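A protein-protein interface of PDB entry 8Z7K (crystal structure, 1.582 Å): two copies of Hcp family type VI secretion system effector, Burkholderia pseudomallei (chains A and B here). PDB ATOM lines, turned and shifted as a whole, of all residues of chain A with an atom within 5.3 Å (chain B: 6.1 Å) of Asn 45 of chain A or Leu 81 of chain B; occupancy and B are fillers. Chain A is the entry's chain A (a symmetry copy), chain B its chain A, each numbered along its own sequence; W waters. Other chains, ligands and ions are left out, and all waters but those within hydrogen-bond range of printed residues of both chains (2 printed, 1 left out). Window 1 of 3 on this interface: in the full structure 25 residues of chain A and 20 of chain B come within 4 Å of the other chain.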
ATOM      1  N   PHE A  43     -13.915 -30.090  18.697  1.00  0.00           N
ATOM      2  CA  PHE A  43     -12.821 -29.211  18.283  1.00  0.00           C
ATOM      3  C   PHE A  43     -13.391 -28.090  17.420  1.00  0.00           C
ATOM      4  O   PHE A  43     -14.423 -28.247  16.776  1.00  0.00           O
ATOM      5  CB  PHE A  43     -11.673 -29.932  17.556  1.00  0.00           C
ATOM      6  CG  PHE A  43     -11.920 -30.178  16.069  1.00  0.00           C
ATOM      7  CD1 PHE A  43     -12.645 -31.288  15.644  1.00  0.00           C
ATOM      8  CD2 PHE A  43     -11.471 -29.265  15.101  1.00  0.00           C
ATOM      9  CE1 PHE A  43     -12.891 -31.476  14.293  1.00  0.00           C
ATOM     10  CE2 PHE A  43     -11.683 -29.480  13.748  1.00  0.00           C
ATOM     11  CZ  PHE A  43     -12.434 -30.566  13.354  1.00  0.00           C
ATOM     12  N   LYS A  44     -12.650 -26.983  17.371  1.00  0.00           N
ATOM     13  CA  LYS A  44     -12.942 -25.876  16.474  1.00  0.00           C
ATOM     14  C   LYS A  44     -11.585 -25.320  16.044  1.00  0.00           C
ATOM     15  O   LYS A  44     -10.832 -24.871  16.900  1.00  0.00           O
ATOM     16  CB  LYS A  44     -13.781 -24.776  17.128  1.00  0.00           C
ATOM     17  CG  LYS A  44     -14.085 -23.604  16.207  1.00  0.00           C
ATOM     18  CD  LYS A  44     -14.705 -22.474  17.025  1.00  0.00           C
ATOM     19  CE  LYS A  44     -14.752 -21.150  16.343  1.00  0.00           C
ATOM     20  NZ  LYS A  44     -15.342 -20.156  17.249  1.00  0.00           N
ATOM     21  N   ASN A  45     -11.245 -25.467  14.772  1.00  0.00           N
ATOM     22  CA  ASN A  45     -10.053 -24.855  14.203  1.00  0.00           C
ATOM     23  C   ASN A  45     -10.488 -23.540  13.552  1.00  0.00           C
ATOM     24  O   ASN A  45     -11.361 -23.512  12.689  1.00  0.00           O
ATOM     25  CB  ASN A  45      -9.395 -25.791  13.208  1.00  0.00           C
ATOM     26  CG  ASN A  45      -8.141 -25.216  12.635  1.00  0.00           C
ATOM     27  OD1 ASN A  45      -7.338 -24.667  13.402  1.00  0.00           O
ATOM     28  ND2 ASN A  45      -7.947 -25.364  11.329  1.00  0.00           N
ATOM     29  N   ASP A  46      -9.907 -22.417  14.020  1.00  0.00           N
ATOM     30  CA  ASP A  46     -10.284 -21.080  13.602  1.00  0.00           C
ATOM     31  C   ASP A  46      -9.030 -20.439  13.026  1.00  0.00           C
ATOM     32  O   ASP A  46      -8.020 -20.404  13.706  1.00  0.00           O
ATOM     33  CB  ASP A  46     -10.825 -20.286  14.778  1.00  0.00           C
ATOM     34  CG  ASP A  46     -11.191 -18.834  14.459  1.00  0.00           C
ATOM     35  OD1 ASP A  46     -10.296 -17.991  14.497  1.00  0.00           O
ATOM     36  OD2 ASP A  46     -12.364 -18.541  14.182  1.00  0.00           O
ATOM     37  N   TYR A  47      -9.077 -19.983  11.777  1.00  0.00           N
ATOM     38  CA  TYR A  47      -7.894 -19.413  11.143  1.00  0.00           C
ATOM     39  C   TYR A  47      -8.306 -18.125  10.412  1.00  0.00           C
ATOM     40  O   TYR A  47      -9.213 -18.134   9.594  1.00  0.00           O
ATOM     41  CB  TYR A  47      -7.242 -20.430  10.210  1.00  0.00           C
ATOM     42  CG  TYR A  47      -5.819 -20.048   9.806  1.00  0.00           C
ATOM     43  CD1 TYR A  47      -5.552 -19.069   8.848  1.00  0.00           C
ATOM     44  CD2 TYR A  47      -4.729 -20.624  10.441  1.00  0.00           C
ATOM     45  CE1 TYR A  47      -4.240 -18.726   8.503  1.00  0.00           C
ATOM     46  CE2 TYR A  47      -3.421 -20.267  10.134  1.00  0.00           C
ATOM     47  CZ  TYR A  47      -3.170 -19.356   9.124  1.00  0.00           C
ATOM     48  OH  TYR A  47      -1.854 -19.055   8.877  1.00  0.00           O
ATOM     49  N   THR A  66      -5.909 -20.677  15.733  1.00  0.00           N
ATOM     50  CA  THR A  66      -6.135 -21.254  17.057  1.00  0.00           C
ATOM     51  C   THR A  66      -7.018 -22.483  16.918  1.00  0.00           C
ATOM     52  O   THR A  66      -7.855 -22.525  16.028  1.00  0.00           O
ATOM     53  CB  THR A  66      -6.771 -20.254  18.009  1.00  0.00           C
ATOM     54  OG1 THR A  66      -8.042 -19.980  17.460  1.00  0.00           O
ATOM     55  CG2 THR A  66      -5.977 -18.976  18.113  1.00  0.00           C
ATOM     56  N   ILE A  67      -6.765 -23.487  17.741  1.00  0.00           N
ATOM     57  CA  ILE A  67      -7.648 -24.650  17.770  1.00  0.00           C
ATOM     58  C   ILE A  67      -8.103 -24.834  19.211  1.00  0.00           C
ATOM     59  O   ILE A  67      -7.262 -24.746  20.118  1.00  0.00           O
ATOM     60  CB  ILE A  67      -7.015 -25.894  17.154  1.00  0.00           C
ATOM     61  CG1 ILE A  67      -8.023 -27.049  17.137  1.00  0.00           C
ATOM     62  CG2 ILE A  67      -5.680 -26.267  17.766  1.00  0.00           C
ATOM     63  CD1 ILE A  67      -7.644 -28.164  16.181  1.00  0.00           C
ATOM     64  N   THR A  68      -9.424 -24.976  19.396  1.00  0.00           N
ATOM     65  CA  THR A  68     -10.000 -25.116  20.729  1.00  0.00           C
ATOM     66  C   THR A  68     -10.467 -26.565  20.859  1.00  0.00           C
ATOM     67  O   THR A  68     -11.212 -27.017  19.985  1.00  0.00           O
ATOM     68  CB  THR A  68     -11.146 -24.131  20.952  1.00  0.00           C
ATOM     69  OG1 THR A  68     -10.632 -22.808  20.765  1.00  0.00           O
ATOM     70  CG2 THR A  68     -11.746 -24.189  22.340  1.00  0.00           C
ATOM     71  N   TYR A 117      -4.742 -33.739  11.447  1.00  0.00           N
ATOM     72  CA  TYR A 117      -4.140 -32.426  11.589  1.00  0.00           C
ATOM     73  C   TYR A 117      -2.797 -32.543  12.291  1.00  0.00           C
ATOM     74  O   TYR A 117      -2.658 -33.340  13.225  1.00  0.00           O
ATOM     75  CB  TYR A 117      -4.930 -31.456  12.472  1.00  0.00           C
ATOM     76  CG  TYR A 117      -6.233 -30.877  11.944  1.00  0.00           C
ATOM     77  CD1 TYR A 117      -7.421 -31.551  12.141  1.00  0.00           C
ATOM     78  CD2 TYR A 117      -6.276 -29.647  11.291  1.00  0.00           C
ATOM     79  CE1 TYR A 117      -8.640 -30.989  11.766  1.00  0.00           C
ATOM     80  CE2 TYR A 117      -7.472 -29.108  10.848  1.00  0.00           C
ATOM     81  CZ  TYR A 117      -8.666 -29.782  11.085  1.00  0.00           C
ATOM     82  OH  TYR A 117      -9.916 -29.344  10.726  1.00  0.00           O
ATOM     83  N   PHE A 119       0.137 -29.637  13.962  1.00  0.00           N
ATOM     84  CA  PHE A 119       0.399 -28.234  14.243  1.00  0.00           C
ATOM     85  C   PHE A 119       1.804 -28.058  14.788  1.00  0.00           C
ATOM     86  O   PHE A 119       2.227 -28.863  15.606  1.00  0.00           O
ATOM     87  CB  PHE A 119      -0.652 -27.692  15.214  1.00  0.00           C
ATOM     88  CG  PHE A 119      -2.084 -27.731  14.681  1.00  0.00           C
ATOM     89  CD1 PHE A 119      -2.534 -26.782  13.768  1.00  0.00           C
ATOM     90  CD2 PHE A 119      -2.968 -28.723  15.073  1.00  0.00           C
ATOM     91  CE1 PHE A 119      -3.819 -26.834  13.277  1.00  0.00           C
ATOM     92  CE2 PHE A 119      -4.265 -28.763  14.594  1.00  0.00           C
ATOM     93  CZ  PHE A 119      -4.696 -27.809  13.708  1.00  0.00           C
ATOM     94  N   TYR A 157      -0.958 -21.678  17.204  1.00  0.00           N
ATOM     95  CA  TYR A 157       0.057 -22.385  16.442  1.00  0.00           C
ATOM     96  C   TYR A 157       0.558 -21.496  15.307  1.00  0.00           C
ATOM     97  O   TYR A 157      -0.060 -20.475  14.992  1.00  0.00           O
ATOM     98  CB  TYR A 157      -0.518 -23.706  15.932  1.00  0.00           C
ATOM     99  CG  TYR A 157      -1.781 -23.564  15.097  1.00  0.00           C
ATOM    100  CD1 TYR A 157      -1.727 -23.204  13.744  1.00  0.00           C
ATOM    101  CD2 TYR A 157      -3.038 -23.825  15.629  1.00  0.00           C
ATOM    102  CE1 TYR A 157      -2.880 -23.085  12.980  1.00  0.00           C
ATOM    103  CE2 TYR A 157      -4.197 -23.698  14.875  1.00  0.00           C
ATOM    104  CZ  TYR A 157      -4.113 -23.358  13.534  1.00  0.00           C
ATOM    105  OH  TYR A 157      -5.235 -23.263  12.778  1.00  0.00           O
ATOM    106  N   TYR A 160       0.883 -25.500  10.110  1.00  0.00           N
ATOM    107  CA  TYR A 160      -0.185 -26.479  10.210  1.00  0.00           C
ATOM    108  C   TYR A 160      -0.202 -27.371   8.978  1.00  0.00           C
ATOM    109  O   TYR A 160       0.254 -26.966   7.931  1.00  0.00           O
ATOM    110  CB  TYR A 160      -1.526 -25.781  10.441  1.00  0.00           C
ATOM    111  CG  TYR A 160      -1.953 -24.903   9.276  1.00  0.00           C
ATOM    112  CD1 TYR A 160      -2.626 -25.440   8.191  1.00  0.00           C
ATOM    113  CD2 TYR A 160      -1.596 -23.558   9.219  1.00  0.00           C
ATOM    114  CE1 TYR A 160      -2.989 -24.655   7.105  1.00  0.00           C
ATOM    115  CE2 TYR A 160      -1.978 -22.755   8.160  1.00  0.00           C
ATOM    116  CZ  TYR A 160      -2.653 -23.310   7.089  1.00  0.00           C
ATOM    117  OH  TYR A 160      -2.998 -22.499   6.051  1.00  0.00           O
ATOM    118  N   LEU A 162      -3.228 -30.364   7.249  1.00  0.00           N
ATOM    119  CA  LEU A 162      -4.464 -31.147   7.275  1.00  0.00           C
ATOM    120  C   LEU A 162      -4.382 -32.112   6.104  1.00  0.00           C
ATOM    121  O   LEU A 162      -4.071 -31.686   5.007  1.00  0.00           O
ATOM    122  CB  LEU A 162      -5.755 -30.325   7.171  1.00  0.00           C
ATOM    123  CG  LEU A 162      -7.106 -31.057   7.147  1.00  0.00           C
ATOM    124  CD1 LEU A 162      -7.322 -31.849   8.417  1.00  0.00           C
ATOM    125  CD2 LEU A 162      -8.304 -30.107   6.940  1.00  0.00           C
ATOM    126  N   SER B  76     -11.608 -31.385  -0.256  1.00  0.00           N
ATOM    127  CA  SER B  76     -11.272 -30.013  -0.590  1.00  0.00           C
ATOM    128  C   SER B  76     -10.831 -29.224   0.647  1.00  0.00           C
ATOM    129  O   SER B  76     -10.169 -28.194   0.469  1.00  0.00           O
ATOM    130  CB  SER B  76     -12.409 -29.307  -1.258  1.00  0.00           C
ATOM    131  OG  SER B  76     -13.557 -29.193  -0.447  1.00  0.00           O
ATOM    132  N   SER B  77     -11.199 -29.705   1.850  1.00  0.00           N
ATOM    133  CA  SER B  77     -10.944 -29.000   3.103  1.00  0.00           C
ATOM    134  C   SER B  77      -9.459 -28.687   3.276  1.00  0.00           C
ATOM    135  O   SER B  77      -9.119 -27.515   3.539  1.00  0.00           O
ATOM    136  CB  SER B  77     -11.504 -29.707   4.286  1.00  0.00           C
ATOM    137  OG  SER B  77     -12.903 -29.844   4.198  1.00  0.00           O
ATOM    138  N   PRO B  78      -8.505 -29.638   3.037  1.00  0.00           N
ATOM    139  CA  PRO B  78      -7.081 -29.311   3.096  1.00  0.00           C
ATOM    140  C   PRO B  78      -6.663 -28.245   2.103  1.00  0.00           C
ATOM    141  O   PRO B  78      -5.821 -27.425   2.472  1.00  0.00           O
ATOM    142  CB  PRO B  78      -6.335 -30.628   2.812  1.00  0.00           C
ATOM    143  CG  PRO B  78      -7.397 -31.682   3.081  1.00  0.00           C
ATOM    144  CD  PRO B  78      -8.709 -31.055   2.709  1.00  0.00           C
ATOM    145  N   GLN B  79      -7.271 -28.269   0.891  1.00  0.00           N
ATOM    146  CA  GLN B  79      -6.927 -27.337  -0.179  1.00  0.00           C
ATOM    147  C   GLN B  79      -7.291 -25.885   0.159  1.00  0.00           C
ATOM    148  O   GLN B  79      -6.450 -25.002  -0.049  1.00  0.00           O
ATOM    149  CB  GLN B  79      -7.563 -27.766  -1.494  1.00  0.00           C
ATOM    150  CG  GLN B  79      -6.932 -29.034  -2.047  1.00  0.00           C
ATOM    151  CD  GLN B  79      -7.683 -29.612  -3.219  1.00  0.00           C
ATOM    152  OE1 GLN B  79      -8.903 -29.817  -3.218  1.00  0.00           O
ATOM    153  NE2 GLN B  79      -6.911 -30.030  -4.189  1.00  0.00           N
ATOM    154  N   PHE B  80      -8.514 -25.679   0.652  1.00  0.00           N
ATOM    155  CA  PHE B  80      -8.961 -24.388   1.142  1.00  0.00           C
ATOM    156  C   PHE B  80      -8.123 -23.931   2.335  1.00  0.00           C
ATOM    157  O   PHE B  80      -7.682 -22.774   2.369  1.00  0.00           O
ATOM    158  CB  PHE B  80     -10.436 -24.483   1.519  1.00  0.00           C
ATOM    159  CG  PHE B  80     -11.409 -24.605   0.358  1.00  0.00           C
ATOM    160  CD1 PHE B  80     -11.425 -23.660  -0.662  1.00  0.00           C
ATOM    161  CD2 PHE B  80     -12.282 -25.678   0.297  1.00  0.00           C
ATOM    162  CE1 PHE B  80     -12.358 -23.753  -1.690  1.00  0.00           C
ATOM    163  CE2 PHE B  80     -13.224 -25.777  -0.735  1.00  0.00           C
ATOM    164  CZ  PHE B  80     -13.264 -24.817  -1.725  1.00  0.00           C
ATOM    165  N   LEU B  81      -7.846 -24.843   3.276  1.00  0.00           N
ATOM    166  CA  LEU B  81      -7.079 -24.481   4.465  1.00  0.00           C
ATOM    167  C   LEU B  81      -5.677 -24.004   4.073  1.00  0.00           C
ATOM    168  O   LEU B  81      -5.155 -23.018   4.611  1.00  0.00           O
ATOM    169  CB  LEU B  81      -7.039 -25.613   5.485  1.00  0.00           C
ATOM    170  CG  LEU B  81      -6.651 -25.225   6.907  1.00  0.00           C
ATOM    171  CD1 LEU B  81      -7.700 -24.344   7.555  1.00  0.00           C
ATOM    172  CD2 LEU B  81      -6.429 -26.489   7.743  1.00  0.00           C
ATOM    173  N   GLN B  82      -5.045 -24.681   3.116  1.00  0.00           N
ATOM    174  CA  GLN B  82      -3.737 -24.238   2.658  1.00  0.00           C
ATOM    175  C   GLN B  82      -3.787 -22.875   1.964  1.00  0.00           C
ATOM    176  O   GLN B  82      -2.920 -22.024   2.216  1.00  0.00           O
ATOM    177  CB  GLN B  82      -3.108 -25.238   1.697  1.00  0.00           C
ATOM    178  CG  GLN B  82      -1.774 -24.768   1.144  1.00  0.00           C
ATOM    179  CD  GLN B  82      -1.085 -25.852   0.352  1.00  0.00           C
ATOM    180  OE1 GLN B  82      -0.798 -26.940   0.843  1.00  0.00           O
ATOM    181  NE2 GLN B  82      -0.773 -25.535  -0.886  1.00  0.00           N
ATOM    182  N   ALA B  83      -4.728 -22.709   1.013  1.00  0.00           N
ATOM    183  CA  ALA B  83      -4.862 -21.462   0.266  1.00  0.00           C
ATOM    184  C   ALA B  83      -4.991 -20.274   1.220  1.00  0.00           C
ATOM    185  O   ALA B  83      -4.410 -19.216   0.966  1.00  0.00           O
ATOM    186  CB  ALA B  83      -6.053 -21.539  -0.686  1.00  0.00           C
ATOM    187  N   LEU B  84      -5.753 -20.473   2.305  1.00  0.00           N
ATOM    188  CA  LEU B  84      -5.979 -19.460   3.321  1.00  0.00           C
ATOM    189  C   LEU B  84      -4.643 -18.979   3.883  1.00  0.00           C
ATOM    190  O   LEU B  84      -4.366 -17.770   3.906  1.00  0.00           O
ATOM    191  CB  LEU B  84      -6.948 -20.005   4.379  1.00  0.00           C
ATOM    192  CG  LEU B  84      -7.128 -19.184   5.662  1.00  0.00           C
ATOM    193  CD1 LEU B  84      -7.554 -17.740   5.397  1.00  0.00           C
ATOM    194  CD2 LEU B  84      -8.103 -19.843   6.594  1.00  0.00           C
ATOM    195  N   GLY B  85      -3.799 -19.932   4.319  1.00  0.00           N
ATOM    196  CA  GLY B  85      -2.539 -19.558   4.936  1.00  0.00           C
ATOM    197  C   GLY B  85      -1.493 -19.016   3.960  1.00  0.00           C
ATOM    198  O   GLY B  85      -0.606 -18.273   4.374  1.00  0.00           O
ATOM    199  N   LYS B  86      -1.580 -19.393   2.681  1.00  0.00           N
ATOM    200  CA  LYS B  86      -0.623 -18.980   1.670  1.00  0.00           C
ATOM    201  C   LYS B  86      -1.100 -17.752   0.892  1.00  0.00           C
ATOM    202  O   LYS B  86      -0.384 -17.304   0.011  1.00  0.00           O
ATOM    203  CB  LYS B  86      -0.410 -20.181   0.739  1.00  0.00           C
ATOM    204  CG  LYS B  86       0.354 -21.333   1.363  1.00  0.00           C
ATOM    205  CD  LYS B  86       0.961 -22.219   0.287  1.00  0.00           C
ATOM    206  CE  LYS B  86       1.758 -23.393   0.736  1.00  0.00           C
ATOM    207  NZ  LYS B  86       2.925 -22.976   1.511  1.00  0.00           N
ATOM    208  N   ILE B 124      -9.356 -16.232   0.378  1.00  0.00           N
ATOM    209  CA  ILE B 124      -9.965 -16.763   1.582  1.00  0.00           C
ATOM    210  C   ILE B 124      -9.454 -15.914   2.750  1.00  0.00           C
ATOM    211  O   ILE B 124      -8.248 -15.657   2.874  1.00  0.00           O
ATOM    212  CB  ILE B 124      -9.661 -18.278   1.746  1.00  0.00           C
ATOM    213  CG1 ILE B 124      -9.919 -19.084   0.467  1.00  0.00           C
ATOM    214  CG2 ILE B 124     -10.484 -18.845   2.898  1.00  0.00           C
ATOM    215  CD1 ILE B 124      -9.573 -20.556   0.544  1.00  0.00           C
ATOM    216  N   MET B 127     -11.477 -19.262   8.040  1.00  0.00           N
ATOM    217  CA  MET B 127     -12.098 -20.588   8.104  1.00  0.00           C
ATOM    218  C   MET B 127     -12.350 -20.977   9.552  1.00  0.00           C
ATOM    219  O   MET B 127     -11.526 -20.724  10.413  1.00  0.00           O
ATOM    220  CB  MET B 127     -11.248 -21.650   7.408  1.00  0.00           C
ATOM    221  CG  MET B 127     -11.353 -21.557   5.903  1.00  0.00           C
ATOM    222  SD  MET B 127     -10.316 -22.748   5.032  1.00  0.00           S
ATOM    223  CE  MET B 127     -11.139 -24.303   5.421  1.00  0.00           C
ATOM    224  N   ASP B 128     -13.498 -21.631   9.795  1.00  0.00           N
ATOM    225  CA  ASP B 128     -13.728 -22.374  11.001  1.00  0.00           C
ATOM    226  C   ASP B 128     -14.144 -23.784  10.612  1.00  0.00           C
ATOM    227  O   ASP B 128     -15.053 -23.929   9.813  1.00  0.00           O
ATOM    228  CB  ASP B 128     -14.821 -21.739  11.830  1.00  0.00           C
ATOM    229  CG  ASP B 128     -14.344 -20.483  12.531  1.00  0.00           C
ATOM    230  OD1 ASP B 128     -13.540 -20.645  13.479  1.00  0.00           O
ATOM    231  OD2 ASP B 128     -14.853 -19.422  12.176  1.00  0.00           O
ATOM    232  N   GLN B 129     -13.472 -24.763  11.209  1.00  0.00           N
ATOM    233  CA  GLN B 129     -13.774 -26.170  10.972  1.00  0.00           C
ATOM    234  C   GLN B 129     -14.114 -26.756  12.317  1.00  0.00           C
ATOM    235  O   GLN B 129     -13.373 -26.564  13.273  1.00  0.00           O
ATOM    236  CB  GLN B 129     -12.515 -26.801  10.391  1.00  0.00           C
ATOM    237  CG  GLN B 129     -11.949 -26.148   9.131  1.00  0.00           C
ATOM    238  CD  GLN B 129     -10.682 -26.829   8.675  1.00  0.00           C
ATOM    239  OE1 GLN B 129      -9.732 -27.020   9.454  1.00  0.00           O
ATOM    240  NE2 GLN B 129     -10.629 -27.176   7.405  1.00  0.00           N
ATOM    241  N   TYR B 130     -15.158 -27.592  12.377  1.00  0.00           N
ATOM    242  CA  TYR B 130     -15.581 -28.011  13.686  1.00  0.00           C
ATOM    243  C   TYR B 130     -16.354 -29.305  13.608  1.00  0.00           C
ATOM    244  O   TYR B 130     -17.008 -29.596  12.611  1.00  0.00           O
ATOM    245  CB  TYR B 130     -16.420 -26.945  14.398  1.00  0.00           C
ATOM    246  CG  TYR B 130     -17.499 -26.264  13.570  1.00  0.00           C
ATOM    247  CD1 TYR B 130     -17.201 -25.151  12.787  1.00  0.00           C
ATOM    248  CD2 TYR B 130     -18.812 -26.724  13.571  1.00  0.00           C
ATOM    249  CE1 TYR B 130     -18.170 -24.518  12.028  1.00  0.00           C
ATOM    250  CE2 TYR B 130     -19.797 -26.092  12.818  1.00  0.00           C
ATOM    251  CZ  TYR B 130     -19.469 -24.998  12.026  1.00  0.00           C
ATOM    252  OH  TYR B 130     -20.429 -24.360  11.282  1.00  0.00           O
HETATM  253  O   HOH W   1     -14.964 -17.528  14.844  1.00  0.00           O
HETATM  254  O   HOH W   2      -0.154 -17.537   7.024  1.00  0.00           O
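The side-chain hydroxyl of Tyr 160 of chain A lies close to the backbone NH of Gly 85 of chain B (3.2 Å). O of Leu 81 of chain B sits at hydrogen-bond distance from OH of Tyr 160 of chain A (2.6 Å). The side-chain amide oxygen of Gln 129 of chain B sits at hydrogen-bond distance from the side-chain hydroxyl of Tyr 117 of chain A, at 2.7 Å. OD1 of Asp 128 of chain B lies close to OD2 of Asp 46 of chain A (2.5 Å). O of Gln 129 of chain B sits at hydrogen-bond distance from N of Asn 45 of chain A (2.8 Å). The backbone NH of Tyr 47 of chain A is in hydrogen-bond range of the backbone carbonyl oxygen of Met 127 of chain B (2.9 Å).
No position is printed for both chains.
Of the 16 printed residues of chain B, 9 touch a printed residue of chain A. Hydrophobic or aromatic side chains of chain A that line the printed part of chain B: Phe 43, Tyr 47, Tyr 117, Tyr 160 and Leu 162. Among the printed residues, 19 pairs touch across the chains. Among the printed residues, no Asp or Glu carboxylate lies within 4 Å of a Lys or Arg side-chain nitrogen of the other chain.
Among the printed residues, merely in contact across the chains: Asn 45 of chain A with Asp 128 of chain B (3.1 Å), Lys 44 of chain A with Asp 128 of chain B (3.2 Å), Lys 44 of chain A with Gln 129 of chain B (3.3 Å), Phe 43 of chain A with Tyr 130 of chain B (3.3 Å), Leu 162 of chain A with Pro 78 of chain B (3.3 Å), Phe 43 of chain A with Gln 129 of chain B (3.4 Å), Asp 46 of chain A with Met 127 of chain B (3.4 Å), Tyr 47 of chain A with Leu 84 of chain B (3.5 Å), Asn 45 of chain A with Met 127 of chain B (3.6 Å), Leu 162 of chain A with Gln 129 of chain B (3.8 Å), Tyr 160 of chain A with Gln 82 of chain B (3.9 Å), Asn 45 of chain A with Leu 81 of chain B (3.9 Å) and Leu 162 of chain A with Leu 81 of chain B (3.9 Å).
Of the printed residues of chain A, Leu 81 of chain B touches Asn 45, Tyr 160 and Leu 162. Of the printed residues of chain A, Met 127 of chain B touches Asn 45, Asp 46 and Tyr 47. Of the printed residues of chain A, Gln 129 of chain B touches Phe 43, Lys 44, Asn 45, Tyr 117 and Leu 162. Printed residues of chain B within 4 Å of Lys 44 of chain A: Asp 128 and Gln 129. Printed residues of chain B within 4 Å of Tyr 160 of chain A: Leu 81 (2.6 Å), Gln 82 (3.9 Å) and Gly 85 (3.2 Å). Of the printed residues of chain B, Phe 43 of chain A touches Gln 129 and Tyr 130. Ser 77 of chain B touches none of the printed residues of chain A. Phe 80 of chain B touches none of the printed residues of chain A.
Water W2 lies within hydrogen-bond range of O of Gly 85 of chain B and OH of Tyr 47 of chain A. Water W1 lies within hydrogen-bond range of OD2 of Asp 46 of chain A (2.9 Å) and OD2 of Asp 128 of chain B (3.3 Å).
SD of Met 127 of chain B lies within hydrogen-bond range of N of Leu 81 of chain B, 3.7 Å away. N of Asp 46 of chain A lies within hydrogen-bond range of O of Thr 66 of chain A, at 2.9 Å. OH of Tyr 157 of chain A is in hydrogen-bond range of OD1 of Asn 45 of chain A, at 2.6 Å. O of Thr 66 of chain A lies close to OD1 of Asn 45 of chain A (3.4 Å). O of Lys 44 of chain A sits at hydrogen-bond distance from N of Thr 68 of chain A (2.9 Å).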
